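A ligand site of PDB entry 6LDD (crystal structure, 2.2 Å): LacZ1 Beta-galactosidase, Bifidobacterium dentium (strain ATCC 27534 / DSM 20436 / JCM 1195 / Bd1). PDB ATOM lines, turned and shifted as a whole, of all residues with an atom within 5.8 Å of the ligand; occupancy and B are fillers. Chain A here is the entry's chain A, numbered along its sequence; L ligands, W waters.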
ATOM      1  N   PHE A 154       7.822  24.542 -29.194  1.00  0.00           N
ATOM      2  CA  PHE A 154       8.244  23.834 -27.986  1.00  0.00           C
ATOM      3  C   PHE A 154       9.556  23.080 -28.182  1.00  0.00           C
ATOM      4  O   PHE A 154       9.693  22.260 -29.088  1.00  0.00           O
ATOM      5  CB  PHE A 154       7.149  22.867 -27.536  1.00  0.00           C
ATOM      6  CG  PHE A 154       7.434  22.185 -26.231  1.00  0.00           C
ATOM      7  CD1 PHE A 154       7.817  22.895 -25.103  1.00  0.00           C
ATOM      8  CD2 PHE A 154       7.307  20.802 -26.132  1.00  0.00           C
ATOM      9  CE1 PHE A 154       8.074  22.243 -23.911  1.00  0.00           C
ATOM     10  CE2 PHE A 154       7.555  20.147 -24.950  1.00  0.00           C
ATOM     11  CZ  PHE A 154       7.939  20.864 -23.834  1.00  0.00           C
ATOM     12  N   MET A 155      10.530  23.392 -27.311  1.00  0.00           N
ATOM     13  CA  MET A 155      11.868  22.808 -27.341  1.00  0.00           C
ATOM     14  C   MET A 155      12.581  23.225 -28.629  1.00  0.00           C
ATOM     15  O   MET A 155      13.341  22.460 -29.225  1.00  0.00           O
ATOM     16  CB  MET A 155      11.804  21.278 -27.230  1.00  0.00           C
ATOM     17  CG  MET A 155      11.568  20.742 -25.814  1.00  0.00           C
ATOM     18  SD  MET A 155      12.972  20.931 -24.704  1.00  0.00           S
ATOM     19  CE  MET A 155      12.270  20.354 -23.157  1.00  0.00           C
ATOM     20  N   ASP A 181       5.054  18.767 -27.758  1.00  0.00           N
ATOM     21  CA  ASP A 181       6.070  18.010 -28.472  1.00  0.00           C
ATOM     22  C   ASP A 181       5.477  16.892 -29.324  1.00  0.00           C
ATOM     23  O   ASP A 181       5.882  15.747 -29.216  1.00  0.00           O
ATOM     24  CB  ASP A 181       7.076  17.413 -27.478  1.00  0.00           C
ATOM     25  CG  ASP A 181       8.263  16.762 -28.154  1.00  0.00           C
ATOM     26  OD1 ASP A 181       8.767  17.325 -29.143  1.00  0.00           O
ATOM     27  OD2 ASP A 181       8.685  15.672 -27.686  1.00  0.00           O
ATOM     28  N   PHE A 182       4.494  17.242 -30.159  1.00  0.00           N
ATOM     29  CA  PHE A 182       4.003  16.322 -31.190  1.00  0.00           C
ATOM     30  C   PHE A 182       3.417  17.148 -32.337  1.00  0.00           C
ATOM     31  O   PHE A 182       2.879  18.227 -32.106  1.00  0.00           O
ATOM     32  CB  PHE A 182       2.975  15.328 -30.625  1.00  0.00           C
ATOM     33  CG  PHE A 182       1.752  15.964 -29.999  1.00  0.00           C
ATOM     34  CD1 PHE A 182       0.640  16.260 -30.768  1.00  0.00           C
ATOM     35  CD2 PHE A 182       1.711  16.216 -28.638  1.00  0.00           C
ATOM     36  CE1 PHE A 182      -0.493  16.825 -30.199  1.00  0.00           C
ATOM     37  CE2 PHE A 182       0.578  16.774 -28.057  1.00  0.00           C
ATOM     38  CZ  PHE A 182      -0.524  17.078 -28.838  1.00  0.00           C
ATOM     39  N   HIS A 381       0.986   7.559 -28.669  1.00  0.00           N
ATOM     40  CA  HIS A 381       0.425   8.613 -29.511  1.00  0.00           C
ATOM     41  C   HIS A 381      -0.419   7.957 -30.583  1.00  0.00           C
ATOM     42  O   HIS A 381      -0.139   6.822 -30.994  1.00  0.00           O
ATOM     43  CB  HIS A 381       1.507   9.487 -30.154  1.00  0.00           C
ATOM     44  CG  HIS A 381       1.731  10.795 -29.461  1.00  0.00           C
ATOM     45  ND1 HIS A 381       0.738  11.756 -29.358  1.00  0.00           N
ATOM     46  CD2 HIS A 381       2.831  11.321 -28.875  1.00  0.00           C
ATOM     47  CE1 HIS A 381       1.227  12.802 -28.712  1.00  0.00           C
ATOM     48  NE2 HIS A 381       2.478  12.577 -28.418  1.00  0.00           N
ATOM     49  N   HIS A 415      -1.627  12.889 -25.900  1.00  0.00           N
ATOM     50  CA  HIS A 415      -2.074  13.873 -24.913  1.00  0.00           C
ATOM     51  C   HIS A 415      -3.446  14.403 -25.316  1.00  0.00           C
ATOM     52  O   HIS A 415      -3.635  15.612 -25.436  1.00  0.00           O
ATOM     53  CB  HIS A 415      -1.095  15.047 -24.824  1.00  0.00           C
ATOM     54  CG  HIS A 415       0.294  14.675 -24.419  1.00  0.00           C
ATOM     55  ND1 HIS A 415       0.594  14.189 -23.163  1.00  0.00           N
ATOM     56  CD2 HIS A 415       1.460  14.725 -25.102  1.00  0.00           C
ATOM     57  CE1 HIS A 415       1.897  13.951 -23.089  1.00  0.00           C
ATOM     58  NE2 HIS A 415       2.441  14.265 -24.249  1.00  0.00           N
ATOM     59  N   VAL A 440      -2.586  20.283 -22.797  1.00  0.00           N
ATOM     60  CA  VAL A 440      -1.134  20.226 -22.790  1.00  0.00           C
ATOM     61  C   VAL A 440      -0.539  21.544 -23.305  1.00  0.00           C
ATOM     62  O   VAL A 440      -1.066  22.139 -24.243  1.00  0.00           O
ATOM     63  CB  VAL A 440      -0.616  19.049 -23.659  1.00  0.00           C
ATOM     64  CG1 VAL A 440      -1.175  19.134 -25.068  1.00  0.00           C
ATOM     65  CG2 VAL A 440       0.916  19.018 -23.694  1.00  0.00           C
ATOM     66  N   ASN A 480      -1.484  17.570 -19.085  1.00  0.00           N
ATOM     67  CA  ASN A 480      -0.105  17.113 -19.156  1.00  0.00           C
ATOM     68  C   ASN A 480       0.897  18.264 -19.080  1.00  0.00           C
ATOM     69  O   ASN A 480       0.858  19.188 -19.891  1.00  0.00           O
ATOM     70  CB  ASN A 480       0.141  16.307 -20.431  1.00  0.00           C
ATOM     71  CG  ASN A 480       1.585  15.831 -20.554  1.00  0.00           C
ATOM     72  OD1 ASN A 480       1.949  14.791 -19.999  1.00  0.00           O
ATOM     73  ND2 ASN A 480       2.401  16.588 -21.290  1.00  0.00           N
ATOM     74  N   GLU A 481       1.779  18.175 -18.091  1.00  0.00           N
ATOM     75  CA  GLU A 481       2.850  19.149 -17.881  1.00  0.00           C
ATOM     76  C   GLU A 481       2.452  20.626 -17.909  1.00  0.00           C
ATOM     77  O   GLU A 481       3.074  21.413 -18.636  1.00  0.00           O
ATOM     78  CB  GLU A 481       3.939  18.913 -18.921  1.00  0.00           C
ATOM     79  CG  GLU A 481       4.550  17.510 -18.866  1.00  0.00           C
ATOM     80  CD  GLU A 481       5.782  17.371 -19.734  1.00  0.00           C
ATOM     81  OE1 GLU A 481       5.889  18.110 -20.735  1.00  0.00           O
ATOM     82  OE2 GLU A 481       6.643  16.524 -19.410  1.00  0.00           O
ATOM     83  N   CYS A 520       5.116  17.718 -15.130  1.00  0.00           N
ATOM     84  CA  CYS A 520       6.440  17.856 -15.721  1.00  0.00           C
ATOM     85  C   CYS A 520       7.522  17.853 -14.657  1.00  0.00           C
ATOM     86  O   CYS A 520       7.251  18.084 -13.473  1.00  0.00           O
ATOM     87  CB  CYS A 520       6.553  19.136 -16.561  1.00  0.00           C
ATOM     88  SG  CYS A 520       6.563  20.666 -15.599  1.00  0.00           S
ATOM     89  N   ASN A 539       6.451  12.941 -14.666  1.00  0.00           N
ATOM     90  CA  ASN A 539       7.352  12.834 -15.795  1.00  0.00           C
ATOM     91  C   ASN A 539       8.750  13.266 -15.369  1.00  0.00           C
ATOM     92  O   ASN A 539       8.943  14.403 -14.965  1.00  0.00           O
ATOM     93  CB  ASN A 539       6.865  13.692 -16.963  1.00  0.00           C
ATOM     94  CG  ASN A 539       5.498  13.283 -17.465  1.00  0.00           C
ATOM     95  OD1 ASN A 539       4.954  12.251 -17.062  1.00  0.00           O
ATOM     96  ND2 ASN A 539       4.931  14.095 -18.359  1.00  0.00           N
ATOM     97  N   TYR A 541      13.077  13.050 -16.291  1.00  0.00           N
ATOM     98  CA  TYR A 541      14.099  12.733 -17.263  1.00  0.00           C
ATOM     99  C   TYR A 541      15.511  12.930 -16.713  1.00  0.00           C
ATOM    100  O   TYR A 541      16.384  13.456 -17.396  1.00  0.00           O
ATOM    101  CB  TYR A 541      13.898  13.579 -18.521  1.00  0.00           C
ATOM    102  CG  TYR A 541      12.666  13.178 -19.305  1.00  0.00           C
ATOM    103  CD1 TYR A 541      11.419  13.698 -18.992  1.00  0.00           C
ATOM    104  CD2 TYR A 541      12.758  12.274 -20.359  1.00  0.00           C
ATOM    105  CE1 TYR A 541      10.301  13.327 -19.693  1.00  0.00           C
ATOM    106  CE2 TYR A 541      11.631  11.907 -21.082  1.00  0.00           C
ATOM    107  CZ  TYR A 541      10.411  12.447 -20.741  1.00  0.00           C
ATOM    108  OH  TYR A 541       9.282  12.085 -21.445  1.00  0.00           O
ATOM    109  N   TYR A 545      17.623  15.006 -19.881  1.00  0.00           N
ATOM    110  CA  TYR A 545      17.541  16.469 -19.975  1.00  0.00           C
ATOM    111  C   TYR A 545      18.370  17.160 -18.881  1.00  0.00           C
ATOM    112  O   TYR A 545      18.609  18.368 -18.928  1.00  0.00           O
ATOM    113  CB  TYR A 545      16.081  16.928 -19.911  1.00  0.00           C
ATOM    114  CG  TYR A 545      15.295  16.650 -21.180  1.00  0.00           C
ATOM    115  CD1 TYR A 545      15.786  17.044 -22.416  1.00  0.00           C
ATOM    116  CD2 TYR A 545      14.062  16.001 -21.134  1.00  0.00           C
ATOM    117  CE1 TYR A 545      15.083  16.798 -23.585  1.00  0.00           C
ATOM    118  CE2 TYR A 545      13.350  15.745 -22.300  1.00  0.00           C
ATOM    119  CZ  TYR A 545      13.859  16.155 -23.518  1.00  0.00           C
ATOM    120  OH  TYR A 545      13.155  15.912 -24.677  1.00  0.00           O
ATOM    121  N   GLU A 576       6.057   9.349 -17.598  1.00  0.00           N
ATOM    122  CA  GLU A 576       7.078   9.546 -18.630  1.00  0.00           C
ATOM    123  C   GLU A 576       8.486   9.426 -18.061  1.00  0.00           C
ATOM    124  O   GLU A 576       8.778   9.949 -16.984  1.00  0.00           O
ATOM    125  CB  GLU A 576       6.944  10.911 -19.314  1.00  0.00           C
ATOM    126  CG  GLU A 576       5.725  11.109 -20.190  1.00  0.00           C
ATOM    127  CD  GLU A 576       5.754  12.451 -20.887  1.00  0.00           C
ATOM    128  OE1 GLU A 576       6.865  13.032 -20.997  1.00  0.00           O
ATOM    129  OE2 GLU A 576       4.677  12.940 -21.289  1.00  0.00           O
ATOM    130  N   ASP A 580      15.978   9.599 -26.162  1.00  0.00           N
ATOM    131  CA  ASP A 580      15.910   9.502 -27.612  1.00  0.00           C
ATOM    132  C   ASP A 580      16.926   8.488 -28.084  1.00  0.00           C
ATOM    133  O   ASP A 580      18.050   8.442 -27.586  1.00  0.00           O
ATOM    134  CB  ASP A 580      16.167  10.860 -28.276  1.00  0.00           C
ATOM    135  CG  ASP A 580      14.991  11.812 -28.111  1.00  0.00           C
ATOM    136  OD1 ASP A 580      14.882  12.440 -27.039  1.00  0.00           O
ATOM    137  OD2 ASP A 580      14.205  11.937 -29.071  1.00  0.00           O
ATOM    138  N   TRP A 621       8.166   6.850 -21.602  1.00  0.00           N
ATOM    139  CA  TRP A 621       7.989   7.628 -22.810  1.00  0.00           C
ATOM    140  C   TRP A 621       9.064   7.167 -23.793  1.00  0.00           C
ATOM    141  O   TRP A 621      10.246   7.239 -23.456  1.00  0.00           O
ATOM    142  CB  TRP A 621       8.095   9.126 -22.506  1.00  0.00           C
ATOM    143  CG  TRP A 621       7.595  10.063 -23.572  1.00  0.00           C
ATOM    144  CD1 TRP A 621       8.345  10.830 -24.409  1.00  0.00           C
ATOM    145  CD2 TRP A 621       6.223  10.320 -23.905  1.00  0.00           C
ATOM    146  NE1 TRP A 621       7.520  11.557 -25.237  1.00  0.00           N
ATOM    147  CE2 TRP A 621       6.225  11.257 -24.954  1.00  0.00           C
ATOM    148  CE3 TRP A 621       5.003   9.842 -23.415  1.00  0.00           C
ATOM    149  CZ2 TRP A 621       5.037  11.736 -25.517  1.00  0.00           C
ATOM    150  CZ3 TRP A 621       3.826  10.310 -23.984  1.00  0.00           C
ATOM    151  CH2 TRP A 621       3.857  11.252 -25.023  1.00  0.00           C
ATOM    152  N   PHE A 626       7.500   9.038 -32.809  1.00  0.00           N
ATOM    153  CA  PHE A 626       6.384   9.750 -33.417  1.00  0.00           C
ATOM    154  C   PHE A 626       6.809  11.101 -33.994  1.00  0.00           C
ATOM    155  O   PHE A 626       7.896  11.600 -33.702  1.00  0.00           O
ATOM    156  CB  PHE A 626       5.260   9.946 -32.401  1.00  0.00           C
ATOM    157  CG  PHE A 626       5.664  10.705 -31.169  1.00  0.00           C
ATOM    158  CD1 PHE A 626       6.117  10.041 -30.043  1.00  0.00           C
ATOM    159  CD2 PHE A 626       5.573  12.088 -31.130  1.00  0.00           C
ATOM    160  CE1 PHE A 626       6.481  10.741 -28.903  1.00  0.00           C
ATOM    161  CE2 PHE A 626       5.936  12.796 -30.002  1.00  0.00           C
ATOM    162  CZ  PHE A 626       6.381  12.118 -28.883  1.00  0.00           C
ATOM    163  N   ARG A 634      15.108  17.119 -32.353  1.00  0.00           N
ATOM    164  CA  ARG A 634      14.165  16.136 -32.872  1.00  0.00           C
ATOM    165  C   ARG A 634      14.668  15.498 -34.172  1.00  0.00           C
ATOM    166  O   ARG A 634      14.524  16.060 -35.260  1.00  0.00           O
ATOM    167  CB  ARG A 634      12.793  16.786 -33.089  1.00  0.00           C
ATOM    168  CG  ARG A 634      12.083  17.132 -31.781  1.00  0.00           C
ATOM    169  CD  ARG A 634      11.792  15.855 -30.996  1.00  0.00           C
ATOM    170  NE  ARG A 634      11.350  16.100 -29.632  1.00  0.00           N
ATOM    171  CZ  ARG A 634      12.106  15.902 -28.551  1.00  0.00           C
ATOM    172  NH1 ARG A 634      13.357  15.460 -28.687  1.00  0.00           N
ATOM    173  NH2 ARG A 634      11.622  16.143 -27.345  1.00  0.00           N
ATOM    174  N   ASN A 638      10.269  12.692 -32.423  1.00  0.00           N
ATOM    175  CA  ASN A 638      10.657  12.207 -31.109  1.00  0.00           C
ATOM    176  C   ASN A 638      11.080  10.740 -31.206  1.00  0.00           C
ATOM    177  O   ASN A 638      10.332   9.915 -31.690  1.00  0.00           O
ATOM    178  CB  ASN A 638       9.497  12.370 -30.128  1.00  0.00           C
ATOM    179  CG  ASN A 638       9.899  12.114 -28.697  1.00  0.00           C
ATOM    180  OD1 ASN A 638      10.329  11.014 -28.350  1.00  0.00           O
ATOM    181  ND2 ASN A 638       9.729  13.123 -27.852  1.00  0.00           N
ATOM    182  N   LYS A 640      12.183   8.746 -28.539  1.00  0.00           N
ATOM    183  CA  LYS A 640      12.197   8.062 -27.243  1.00  0.00           C
ATOM    184  C   LYS A 640      11.331   6.798 -27.238  1.00  0.00           C
ATOM    185  O   LYS A 640      11.141   6.169 -26.189  1.00  0.00           O
ATOM    186  CB  LYS A 640      11.726   9.008 -26.124  1.00  0.00           C
ATOM    187  CG  LYS A 640      12.656  10.191 -25.865  1.00  0.00           C
ATOM    188  CD  LYS A 640      12.256  10.916 -24.580  1.00  0.00           C
ATOM    189  CE  LYS A 640      13.122  12.143 -24.337  1.00  0.00           C
ATOM    190  NZ  LYS A 640      12.910  13.217 -25.355  1.00  0.00           N
HETATM  191  N1  LIG L   1       7.098  15.588 -22.024  1.00  0.00           N
HETATM  192  C1  LIG L   1       9.606  18.247 -21.720  1.00  0.00           C
HETATM  193  C2  LIG L   1       5.829  15.574 -22.745  1.00  0.00           C
HETATM  194  C3  LIG L   1       5.905  14.754 -24.028  1.00  0.00           C
HETATM  195  C4  LIG L   1       7.232  14.949 -24.758  1.00  0.00           C
HETATM  196  C5  LIG L   1       8.376  14.643 -23.798  1.00  0.00           C
HETATM  197  C6  LIG L   1       9.704  14.573 -24.511  1.00  0.00           C
HETATM  198  C7  LIG L   1       8.327  15.762 -22.766  1.00  0.00           C
HETATM  199  C8  LIG L   1       9.527  15.746 -21.825  1.00  0.00           C
HETATM  200  C9  LIG L   1       9.515  16.969 -20.920  1.00  0.00           C
HETATM  201  O1  LIG L   1       4.814  15.099 -24.891  1.00  0.00           O
HETATM  202  O2  LIG L   1       7.305  14.083 -25.896  1.00  0.00           O
HETATM  203  O3  LIG L   1      10.129  13.497 -24.896  1.00  0.00           O
HETATM  204  O4  LIG L   1      10.426  15.664 -24.740  1.00  0.00           O
HETATM  205  O   HOH W   1       4.352  17.805 -25.159  1.00  0.00           O
HETATM  206  O   HOH W   2       4.215  14.508 -27.319  1.00  0.00           O
HETATM  207  O   HOH W   3       9.068  16.552 -17.738  1.00  0.00           O
HETATM  208  O   HOH W   4      11.346  17.799 -18.401  1.00  0.00           O
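An oxygen (O1) of the ligand sits at hydrogen-bond distance from a ring nitrogen (NE2) of His 415.
The indole nitrogen of Trp 621 lies within hydrogen-bond range of an oxygen (O2) of the ligand, 2.6 Å away.
An oxygen (O4) of the ligand sits at hydrogen-bond distance from the side-chain hydroxyl of Tyr 545 (2.7 Å).
An oxygen (O2) of the ligand sits at hydrogen-bond distance from the side-chain carboxylate of Asp 181, at 2.8 Å.
The side-chain carboxylate (OE1) of Glu 576 lies within salt-bridge range of a nitrogen (N1) of the ligand.
A nitrogen (N1) of the ligand lies within salt-bridge range of the side-chain carboxylate (OE2) of Glu 481, at 2.8 Å.
O3 of the ligand is in salt-bridge range of NZ of Lys 640, 2.8 Å away.
The guanidinium group of Arg 634 lies within salt-bridge range of an oxygen (O4) of the ligand (2.9 Å).
The side-chain amide nitrogen (ND2) of Asn 638 is in hydrogen-bond range of an oxygen (O3) of the ligand.
ND1 of His 415 lies close to OD1 of Asn 480, at 3.5 Å.
The guanidinium group of Arg 634 is in hydrogen-bond range of the side-chain hydroxyl of Tyr 545 (3.1 Å).
The side-chain carboxylate (OD1) of Asp 181 lies within salt-bridge range of the guanidinium group (NE) of Arg 634, 2.9 Å away.
ND2 of Asn 638 sits at hydrogen-bond distance from OD2 of Asp 181 (2.8 Å).
OE2 of Glu 481 is in hydrogen-bond range of ND2 of Asn 539 (3.2 Å).
OD1 of Asn 638 lies within hydrogen-bond range of N of Lys 640, 2.9 Å away.
OD2 of Asp 580 lies within salt-bridge range of NH1 of Arg 634 (3.6 Å).
The backbone NH of Asn 638 sits at hydrogen-bond distance from the backbone carbonyl oxygen of Phe 626 (2.9 Å).
CZ of Phe 154 touches C1 of the ligand, at 3.8 Å.
Met 155 touches the ligand.
Asn 480 touches the ligand (ND2 to C2, 3.9 Å).
CE1 of Tyr 541 touches C8 of the ligand, 3.3 Å away.
CZ of Phe 626 touches O2 of the ligand, 3.7 Å away.
Hydrophobic or aromatic side chains that line the ligand: Phe 154, Met 155, His 415, Tyr 541, Tyr 545, Trp 621 and Phe 626.
Within 4 Å of the ligand: Phe 154, Met 155, Asp 181, His 415, Asn 480, Glu 481, Tyr 541, Tyr 545, Glu 576, Trp 621, Phe 626, Arg 634, Asn 638 and Lys 640.
Along chain A the residues within 4 Å of the ligand span positions 154 to 640.
Water W2 lies within hydrogen-bond range of O1 of the ligand (2.6 Å), O of Asp 181 (2.8 Å) and NE2 of His 381 (2.8 Å).
Water W1 lies within hydrogen-bond range of an oxygen (O1) of the ligand and the backbone NH of Asp 181.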
